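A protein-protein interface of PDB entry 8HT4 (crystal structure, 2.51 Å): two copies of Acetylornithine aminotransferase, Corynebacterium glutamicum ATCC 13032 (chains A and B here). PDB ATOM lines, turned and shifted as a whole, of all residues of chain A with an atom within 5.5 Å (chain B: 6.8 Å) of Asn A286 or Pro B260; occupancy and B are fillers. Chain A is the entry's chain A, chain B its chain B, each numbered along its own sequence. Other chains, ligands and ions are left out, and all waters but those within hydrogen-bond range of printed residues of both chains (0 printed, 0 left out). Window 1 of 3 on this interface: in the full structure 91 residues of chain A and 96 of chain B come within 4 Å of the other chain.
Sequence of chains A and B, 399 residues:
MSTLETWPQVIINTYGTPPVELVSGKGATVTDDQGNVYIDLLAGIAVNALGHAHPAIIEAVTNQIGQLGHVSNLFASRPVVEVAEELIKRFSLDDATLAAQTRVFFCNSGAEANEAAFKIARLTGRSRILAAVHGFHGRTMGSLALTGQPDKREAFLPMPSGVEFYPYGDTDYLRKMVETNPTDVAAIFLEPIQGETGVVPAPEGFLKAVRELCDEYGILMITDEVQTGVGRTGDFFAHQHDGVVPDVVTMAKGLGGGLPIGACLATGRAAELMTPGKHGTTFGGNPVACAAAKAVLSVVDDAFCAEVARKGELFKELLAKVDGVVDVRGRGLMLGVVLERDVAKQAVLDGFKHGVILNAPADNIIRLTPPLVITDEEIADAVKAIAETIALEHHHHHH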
ATOM      1  N   GLY A  69      -8.047  24.785  10.318  1.00  0.00           N
ATOM      2  CA  GLY A  69      -8.423  23.542   9.629  1.00  0.00           C
ATOM      3  C   GLY A  69      -9.536  23.808   8.636  1.00  0.00           C
ATOM      4  O   GLY A  69      -9.596  24.934   8.095  1.00  0.00           O
ATOM      5  N   HIS A  70     -10.416  22.825   8.433  1.00  0.00           N
ATOM      6  CA  HIS A  70     -11.474  22.864   7.392  1.00  0.00           C
ATOM      7  C   HIS A  70     -12.245  24.166   7.484  1.00  0.00           C
ATOM      8  O   HIS A  70     -12.723  24.554   8.585  1.00  0.00           O
ATOM      9  CB  HIS A  70     -12.469  21.721   7.480  1.00  0.00           C
ATOM     10  CG  HIS A  70     -13.666  21.914   6.610  1.00  0.00           C
ATOM     11  ND1 HIS A  70     -13.727  21.452   5.304  1.00  0.00           N
ATOM     12  CD2 HIS A  70     -14.868  22.483   6.879  1.00  0.00           C
ATOM     13  CE1 HIS A  70     -14.917  21.730   4.806  1.00  0.00           C
ATOM     14  NE2 HIS A  70     -15.631  22.383   5.748  1.00  0.00           N
ATOM     15  N   PRO A  79      -3.648  28.160   1.457  1.00  0.00           N
ATOM     16  CA  PRO A  79      -2.990  26.981   0.880  1.00  0.00           C
ATOM     17  C   PRO A  79      -3.577  26.393  -0.415  1.00  0.00           C
ATOM     18  O   PRO A  79      -2.766  26.119  -1.287  1.00  0.00           O
ATOM     19  CB  PRO A  79      -3.079  25.935   1.997  1.00  0.00           C
ATOM     20  CG  PRO A  79      -3.166  26.771   3.248  1.00  0.00           C
ATOM     21  CD  PRO A  79      -4.039  27.945   2.857  1.00  0.00           C
ATOM     22  N   VAL A  80      -4.904  26.222  -0.542  1.00  0.00           N
ATOM     23  CA  VAL A  80      -5.502  25.608  -1.776  1.00  0.00           C
ATOM     24  C   VAL A  80      -4.984  26.335  -3.017  1.00  0.00           C
ATOM     25  O   VAL A  80      -4.702  25.672  -4.007  1.00  0.00           O
ATOM     26  CB  VAL A  80      -7.041  25.627  -1.880  1.00  0.00           C
ATOM     27  CG1 VAL A  80      -7.514  24.455  -2.733  1.00  0.00           C
ATOM     28  CG2 VAL A  80      -7.758  25.650  -0.553  1.00  0.00           C
ATOM     29  N   ASN A 108     -10.494  14.673  -2.301  1.00  0.00           N
ATOM     30  CA  ASN A 108      -9.860  13.967  -1.145  1.00  0.00           C
ATOM     31  C   ASN A 108      -9.232  12.620  -1.529  1.00  0.00           C
ATOM     32  O   ASN A 108      -8.615  11.998  -0.648  1.00  0.00           O
ATOM     33  CB  ASN A 108     -10.864  13.758  -0.004  1.00  0.00           C
ATOM     34  CG  ASN A 108     -11.523  15.065   0.367  1.00  0.00           C
ATOM     35  OD1 ASN A 108     -10.859  15.961   0.879  1.00  0.00           O
ATOM     36  ND2 ASN A 108     -12.780  15.229  -0.020  1.00  0.00           N
ATOM     37  N   LEU A 259      -1.195  12.902   3.676  1.00  0.00           N
ATOM     38  CA  LEU A 259      -2.498  13.480   4.037  1.00  0.00           C
ATOM     39  C   LEU A 259      -3.466  13.299   2.871  1.00  0.00           C
ATOM     40  O   LEU A 259      -3.050  13.468   1.721  1.00  0.00           O
ATOM     41  CB  LEU A 259      -2.346  14.933   4.488  1.00  0.00           C
ATOM     42  CG  LEU A 259      -2.218  15.120   5.997  1.00  0.00           C
ATOM     43  CD1 LEU A 259      -0.785  15.428   6.381  1.00  0.00           C
ATOM     44  CD2 LEU A 259      -3.154  16.204   6.496  1.00  0.00           C
ATOM     45  N   PRO A 260      -4.729  12.929   3.146  1.00  0.00           N
ATOM     46  CA  PRO A 260      -5.734  12.750   2.102  1.00  0.00           C
ATOM     47  C   PRO A 260      -6.011  13.940   1.163  1.00  0.00           C
ATOM     48  O   PRO A 260      -6.543  14.912   1.610  1.00  0.00           O
ATOM     49  CB  PRO A 260      -6.971  12.318   2.911  1.00  0.00           C
ATOM     50  CG  PRO A 260      -6.744  12.845   4.294  1.00  0.00           C
ATOM     51  CD  PRO A 260      -5.257  12.708   4.487  1.00  0.00           C
ATOM     52  N   PHE A 283     -14.676  18.782   1.927  1.00  0.00           N
ATOM     53  CA  PHE A 283     -13.256  18.857   2.351  1.00  0.00           C
ATOM     54  C   PHE A 283     -12.343  19.402   1.255  1.00  0.00           C
ATOM     55  O   PHE A 283     -11.182  19.637   1.574  1.00  0.00           O
ATOM     56  CB  PHE A 283     -12.780  17.523   2.927  1.00  0.00           C
ATOM     57  CG  PHE A 283     -13.448  17.029   4.180  1.00  0.00           C
ATOM     58  CD1 PHE A 283     -13.663  17.869   5.258  1.00  0.00           C
ATOM     59  CD2 PHE A 283     -13.829  15.704   4.289  1.00  0.00           C
ATOM     60  CE1 PHE A 283     -14.261  17.394   6.410  1.00  0.00           C
ATOM     61  CE2 PHE A 283     -14.417  15.230   5.447  1.00  0.00           C
ATOM     62  CZ  PHE A 283     -14.634  16.076   6.506  1.00  0.00           C
ATOM     63  N   GLY A 284     -12.855  19.584   0.039  1.00  0.00           N
ATOM     64  CA  GLY A 284     -12.074  20.109  -1.094  1.00  0.00           C
ATOM     65  C   GLY A 284     -11.293  21.355  -0.747  1.00  0.00           C
ATOM     66  O   GLY A 284     -11.890  22.323  -0.319  1.00  0.00           O
ATOM     67  N   GLY A 285      -9.975  21.304  -0.872  1.00  0.00           N
ATOM     68  CA  GLY A 285      -9.134  22.438  -0.481  1.00  0.00           C
ATOM     69  C   GLY A 285      -8.835  22.474   0.993  1.00  0.00           C
ATOM     70  O   GLY A 285      -8.638  23.558   1.509  1.00  0.00           O
ATOM     71  N   ASN A 286      -8.836  21.324   1.651  1.00  0.00           N
ATOM     72  CA  ASN A 286      -8.449  21.278   3.076  1.00  0.00           C
ATOM     73  C   ASN A 286      -7.145  22.042   3.296  1.00  0.00           C
ATOM     74  O   ASN A 286      -6.142  21.674   2.717  1.00  0.00           O
ATOM     75  CB  ASN A 286      -8.355  19.853   3.610  1.00  0.00           C
ATOM     76  CG  ASN A 286      -8.361  19.794   5.116  1.00  0.00           C
ATOM     77  OD1 ASN A 286      -9.387  20.051   5.728  1.00  0.00           O
ATOM     78  ND2 ASN A 286      -7.233  19.452   5.708  1.00  0.00           N
ATOM     79  N   PRO A 287      -7.149  23.053   4.178  1.00  0.00           N
ATOM     80  CA  PRO A 287      -5.942  23.816   4.472  1.00  0.00           C
ATOM     81  C   PRO A 287      -4.721  23.051   4.994  1.00  0.00           C
ATOM     82  O   PRO A 287      -3.660  23.491   4.718  1.00  0.00           O
ATOM     83  CB  PRO A 287      -6.473  24.896   5.433  1.00  0.00           C
ATOM     84  CG  PRO A 287      -7.946  24.971   5.152  1.00  0.00           C
ATOM     85  CD  PRO A 287      -8.325  23.535   4.892  1.00  0.00           C
ATOM     86  N   VAL A 288      -4.918  21.927   5.677  1.00  0.00           N
ATOM     87  CA  VAL A 288      -3.809  21.146   6.293  1.00  0.00           C
ATOM     88  C   VAL A 288      -3.210  20.216   5.246  1.00  0.00           C
ATOM     89  O   VAL A 288      -1.996  20.105   5.187  1.00  0.00           O
ATOM     90  CB  VAL A 288      -4.297  20.411   7.564  1.00  0.00           C
ATOM     91  CG1 VAL A 288      -3.187  19.676   8.289  1.00  0.00           C
ATOM     92  CG2 VAL A 288      -5.011  21.356   8.513  1.00  0.00           C
ATOM     93  N   ALA A 289      -4.057  19.592   4.451  1.00  0.00           N
ATOM     94  CA  ALA A 289      -3.610  18.684   3.387  1.00  0.00           C
ATOM     95  C   ALA A 289      -2.986  19.492   2.252  1.00  0.00           C
ATOM     96  O   ALA A 289      -2.091  18.971   1.602  1.00  0.00           O
ATOM     97  CB  ALA A 289      -4.806  17.903   2.933  1.00  0.00           C
ATOM     98  N   CYS A 290      -3.454  20.717   2.056  1.00  0.00           N
ATOM     99  CA  CYS A 290      -2.935  21.606   0.994  1.00  0.00           C
ATOM    100  C   CYS A 290      -1.642  22.237   1.521  1.00  0.00           C
ATOM    101  O   CYS A 290      -0.793  22.607   0.726  1.00  0.00           O
ATOM    102  CB  CYS A 290      -4.007  22.604   0.550  1.00  0.00           C
ATOM    103  SG  CYS A 290      -5.313  21.948  -0.510  1.00  0.00           S
ATOM    104  N   ALA A 291      -1.491  22.306   2.834  1.00  0.00           N
ATOM    105  CA  ALA A 291      -0.220  22.766   3.414  1.00  0.00           C
ATOM    106  C   ALA A 291       0.832  21.688   3.160  1.00  0.00           C
ATOM    107  O   ALA A 291       1.935  22.047   2.739  1.00  0.00           O
ATOM    108  CB  ALA A 291      -0.383  23.059   4.879  1.00  0.00           C
ATOM    109  N   VAL B  47     -18.744  20.858  10.184  1.00  0.00           N
ATOM    110  CA  VAL B  47     -17.486  20.055  10.119  1.00  0.00           C
ATOM    111  C   VAL B  47     -16.688  20.235  11.419  1.00  0.00           C
ATOM    112  O   VAL B  47     -16.202  19.218  11.957  1.00  0.00           O
ATOM    113  CB  VAL B  47     -16.649  20.446   8.881  1.00  0.00           C
ATOM    114  CG1 VAL B  47     -15.234  19.899   8.953  1.00  0.00           C
ATOM    115  CG2 VAL B  47     -17.304  20.022   7.584  1.00  0.00           C
ATOM    116  N   CYS B 107     -12.933   5.969   4.935  1.00  0.00           N
ATOM    117  CA  CYS B 107     -12.729   6.682   3.641  1.00  0.00           C
ATOM    118  C   CYS B 107     -12.477   8.160   3.954  1.00  0.00           C
ATOM    119  O   CYS B 107     -12.043   8.442   5.091  1.00  0.00           O
ATOM    120  CB  CYS B 107     -13.903   6.437   2.700  1.00  0.00           C
ATOM    121  SG  CYS B 107     -15.513   6.799   3.449  1.00  0.00           S
ATOM    122  N   ASN B 108     -12.700   9.080   3.016  1.00  0.00           N
ATOM    123  CA  ASN B 108     -12.166  10.469   3.136  1.00  0.00           C
ATOM    124  C   ASN B 108     -13.266  11.537   3.018  1.00  0.00           C
ATOM    125  O   ASN B 108     -12.868  12.725   2.981  1.00  0.00           O
ATOM    126  CB  ASN B 108     -11.089  10.687   2.082  1.00  0.00           C
ATOM    127  CG  ASN B 108     -10.141   9.508   2.021  1.00  0.00           C
ATOM    128  OD1 ASN B 108      -9.449   9.226   2.989  1.00  0.00           O
ATOM    129  ND2 ASN B 108     -10.134   8.789   0.914  1.00  0.00           N
ATOM    130  N   SER B 109     -14.558  11.157   2.980  1.00  0.00           N
ATOM    131  CA  SER B 109     -15.694  12.079   2.716  1.00  0.00           C
ATOM    132  C   SER B 109     -17.054  11.404   2.949  1.00  0.00           C
ATOM    133  O   SER B 109     -17.154  10.193   2.912  1.00  0.00           O
ATOM    134  CB  SER B 109     -15.627  12.615   1.289  1.00  0.00           C
ATOM    135  OG  SER B 109     -15.889  11.598   0.322  1.00  0.00           O
ATOM    136  N   GLY B 256     -13.874  14.245  11.568  1.00  0.00           N
ATOM    137  CA  GLY B 256     -12.492  14.671  11.284  1.00  0.00           C
ATOM    138  C   GLY B 256     -12.054  15.911  12.054  1.00  0.00           C
ATOM    139  O   GLY B 256     -10.848  16.120  12.117  1.00  0.00           O
ATOM    140  N   GLY B 258     -12.044  18.993  11.116  1.00  0.00           N
ATOM    141  CA  GLY B 258     -11.272  19.856  10.205  1.00  0.00           C
ATOM    142  C   GLY B 258     -10.350  19.089   9.281  1.00  0.00           C
ATOM    143  O   GLY B 258      -9.777  19.721   8.369  1.00  0.00           O
ATOM    144  N   LEU B 259     -10.165  17.787   9.507  1.00  0.00           N
ATOM    145  CA  LEU B 259      -9.320  16.938   8.629  1.00  0.00           C
ATOM    146  C   LEU B 259     -10.249  16.049   7.821  1.00  0.00           C
ATOM    147  O   LEU B 259     -11.309  15.668   8.307  1.00  0.00           O
ATOM    148  CB  LEU B 259      -8.309  16.153   9.465  1.00  0.00           C
ATOM    149  CG  LEU B 259      -6.893  16.746   9.486  1.00  0.00           C
ATOM    150  CD1 LEU B 259      -6.912  18.250   9.665  1.00  0.00           C
ATOM    151  CD2 LEU B 259      -6.033  16.122  10.560  1.00  0.00           C
ATOM    152  N   PRO B 260      -9.916  15.754   6.543  1.00  0.00           N
ATOM    153  CA  PRO B 260     -10.732  14.868   5.718  1.00  0.00           C
ATOM    154  C   PRO B 260     -10.770  13.443   6.281  1.00  0.00           C
ATOM    155  O   PRO B 260      -9.752  12.894   6.584  1.00  0.00           O
ATOM    156  CB  PRO B 260     -10.033  14.880   4.354  1.00  0.00           C
ATOM    157  CG  PRO B 260      -9.204  16.141   4.390  1.00  0.00           C
ATOM    158  CD  PRO B 260      -8.728  16.232   5.820  1.00  0.00           C
ATOM    159  N   ILE B 261     -11.975  12.902   6.392  1.00  0.00           N
ATOM    160  CA  ILE B 261     -12.258  11.529   6.877  1.00  0.00           C
ATOM    161  C   ILE B 261     -13.731  11.213   6.586  1.00  0.00           C
ATOM    162  O   ILE B 261     -14.582  12.119   6.543  1.00  0.00           O
ATOM    163  CB  ILE B 261     -11.908  11.373   8.368  1.00  0.00           C
ATOM    164  CG1 ILE B 261     -11.808   9.905   8.775  1.00  0.00           C
ATOM    165  CG2 ILE B 261     -12.892  12.134   9.244  1.00  0.00           C
ATOM    166  CD1 ILE B 261     -11.476   9.684  10.237  1.00  0.00           C
ATOM    167  N   GLY B 262     -13.997   9.940   6.357  1.00  0.00           N
ATOM    168  CA  GLY B 262     -15.356   9.391   6.235  1.00  0.00           C
ATOM    169  C   GLY B 262     -15.380   7.975   6.764  1.00  0.00           C
ATOM    170  O   GLY B 262     -14.291   7.356   6.990  1.00  0.00           O
ATOM    171  N   ASN B 286      -6.289   6.795   7.284  1.00  0.00           N
ATOM    172  CA  ASN B 286      -5.175   7.782   7.401  1.00  0.00           C
ATOM    173  C   ASN B 286      -4.848   8.003   8.875  1.00  0.00           C
ATOM    174  O   ASN B 286      -5.715   8.364   9.679  1.00  0.00           O
ATOM    175  CB  ASN B 286      -5.518   9.127   6.756  1.00  0.00           C
ATOM    176  CG  ASN B 286      -4.337  10.070   6.684  1.00  0.00           C
ATOM    177  OD1 ASN B 286      -4.154  10.927   7.564  1.00  0.00           O
ATOM    178  ND2 ASN B 286      -3.530   9.903   5.647  1.00  0.00           N
ATOM    179  N   VAL B 288      -3.288  10.408  10.396  1.00  0.00           N
ATOM    180  CA  VAL B 288      -3.354  11.815  10.902  1.00  0.00           C
ATOM    181  C   VAL B 288      -4.830  12.155  11.124  1.00  0.00           C
ATOM    182  O   VAL B 288      -5.197  12.552  12.233  1.00  0.00           O
ATOM    183  CB  VAL B 288      -2.635  12.816   9.974  1.00  0.00           C
ATOM    184  CG1 VAL B 288      -2.720  14.244  10.503  1.00  0.00           C
ATOM    185  CG2 VAL B 288      -1.180  12.426   9.754  1.00  0.00           C
ATOM    186  N   ALA B 289      -5.671  11.904  10.131  1.00  0.00           N
ATOM    187  CA  ALA B 289      -7.127  12.165  10.191  1.00  0.00           C
ATOM    188  C   ALA B 289      -7.770  11.394  11.352  1.00  0.00           C
ATOM    189  O   ALA B 289      -8.593  11.980  12.106  1.00  0.00           O
ATOM    190  CB  ALA B 289      -7.744  11.806   8.864  1.00  0.00           C
ATOM    191  N   CYS B 290      -7.455  10.107  11.463  1.00  0.00           N
ATOM    192  CA  CYS B 290      -7.987   9.227  12.540  1.00  0.00           C
ATOM    193  C   CYS B 290      -7.478   9.718  13.915  1.00  0.00           C
ATOM    194  O   CYS B 290      -8.243   9.633  14.904  1.00  0.00           O
ATOM    195  CB  CYS B 290      -7.645   7.765  12.254  1.00  0.00           C
ATOM    196  SG  CYS B 290      -8.529   7.077  10.822  1.00  0.00           S
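The backbone carbonyl oxygen of Gly B258 is in hydrogen-bond range of the backbone NH of His A70, 3.2 Å away. The backbone carbonyl oxygen (O) of Gly B258 lies close to the side-chain amide oxygen (OD1) of Asn A286, at 2.7 Å.
The backbone NH of Val A288 lies close to the side-chain amide nitrogen of Asn A286 (3.4 Å). ND2 of Asn A286 sits close to N of Ala A289, at 3.4 Å. O of Asn A286 sits close to SG of Cys A290 (3.3 Å). The backbone NH (N) of Val B288 lies within hydrogen-bond range of the side-chain amide oxygen (OD1) of Asn B286 (3.0 Å). The backbone NH of Ala B289 lies within hydrogen-bond range of the side-chain amide oxygen of Asn B286, at 3.1 Å. SG of Cys B290 lies close to O of Asn B286 (3.3 Å).
CD2 of His A70 touches CG1 of Val B47 (3.3 Å). Asn B108 touches Asn A108 (CB to CB, 3.7 Å). Pro B260 touches Asn A108 (CB to OD1, 3.7 Å). CG of Pro A260 touches O of Pro B260, at 3.8 Å. Asn B286 touches Pro A260. CG1 of Val B47 touches CE1 of Phe A283 (3.7 Å). Asn B108 touches Phe A283. Leu B259 touches Phe A283. Phe A283 touches Pro B260 (CD2 to CA, 3.5 Å). Asn A286 touches Pro B260 (ND2 to CD, 3.6 Å).
Asn A286 touches just these residues of chain B: Gly B258 (2.7 Å) and Pro B260 (3.6 Å). Of chain A, only Asn A108, Pro A260, Phe A283 and Asn A286 come within 4 Å of Pro B260. Of the printed residues of chain A, Val B47 touches His A70 and Phe A283. Of the printed residues of chain B, Phe A283 touches Val B47, Asn B108, Leu B259, Pro B260 and Ile B261. Gly A69 touches none of the printed residues of chain B. Gly A284 touches none of the printed residues of chain B. The nearest residue of chain B that does not touch Asn A286 is Leu B259 (4.1 Å). The nearest residue of chain A that does not touch Pro B260 is Ala A289 (5.0 Å).
Printed residues of chain B that touch a printed residue of chain A: Val B47, Asn B108, Gly B258, Leu B259, Pro B260, Ile B261 and Asn B286. Hydrophobic or aromatic side chains of chain B within 4 Å of the printed part of chain A: Val B47, Leu B259 and Pro B260. Hydrophobic or aromatic side chains of chain A within 4 Å of the printed part of chain B: His A70, Pro A260, Phe A283 and Val A288. Among the printed residues, 15 pairs touch across the chains.
Asn A108 touches its own counterpart, Asn B108. Asn A108 touches Pro B260, and with the chains exchanged Pro A260 touches Asn B108. Pro A260 touches its own counterpart, Pro B260. Pro A260 touches Asn B286, and with the chains exchanged Asn A286 touches Pro B260. 7 positions are printed for both chains. Of the 15 pairs that touch across the chains among the printed residues, 6 have their exchanged pair printed and touching as well.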
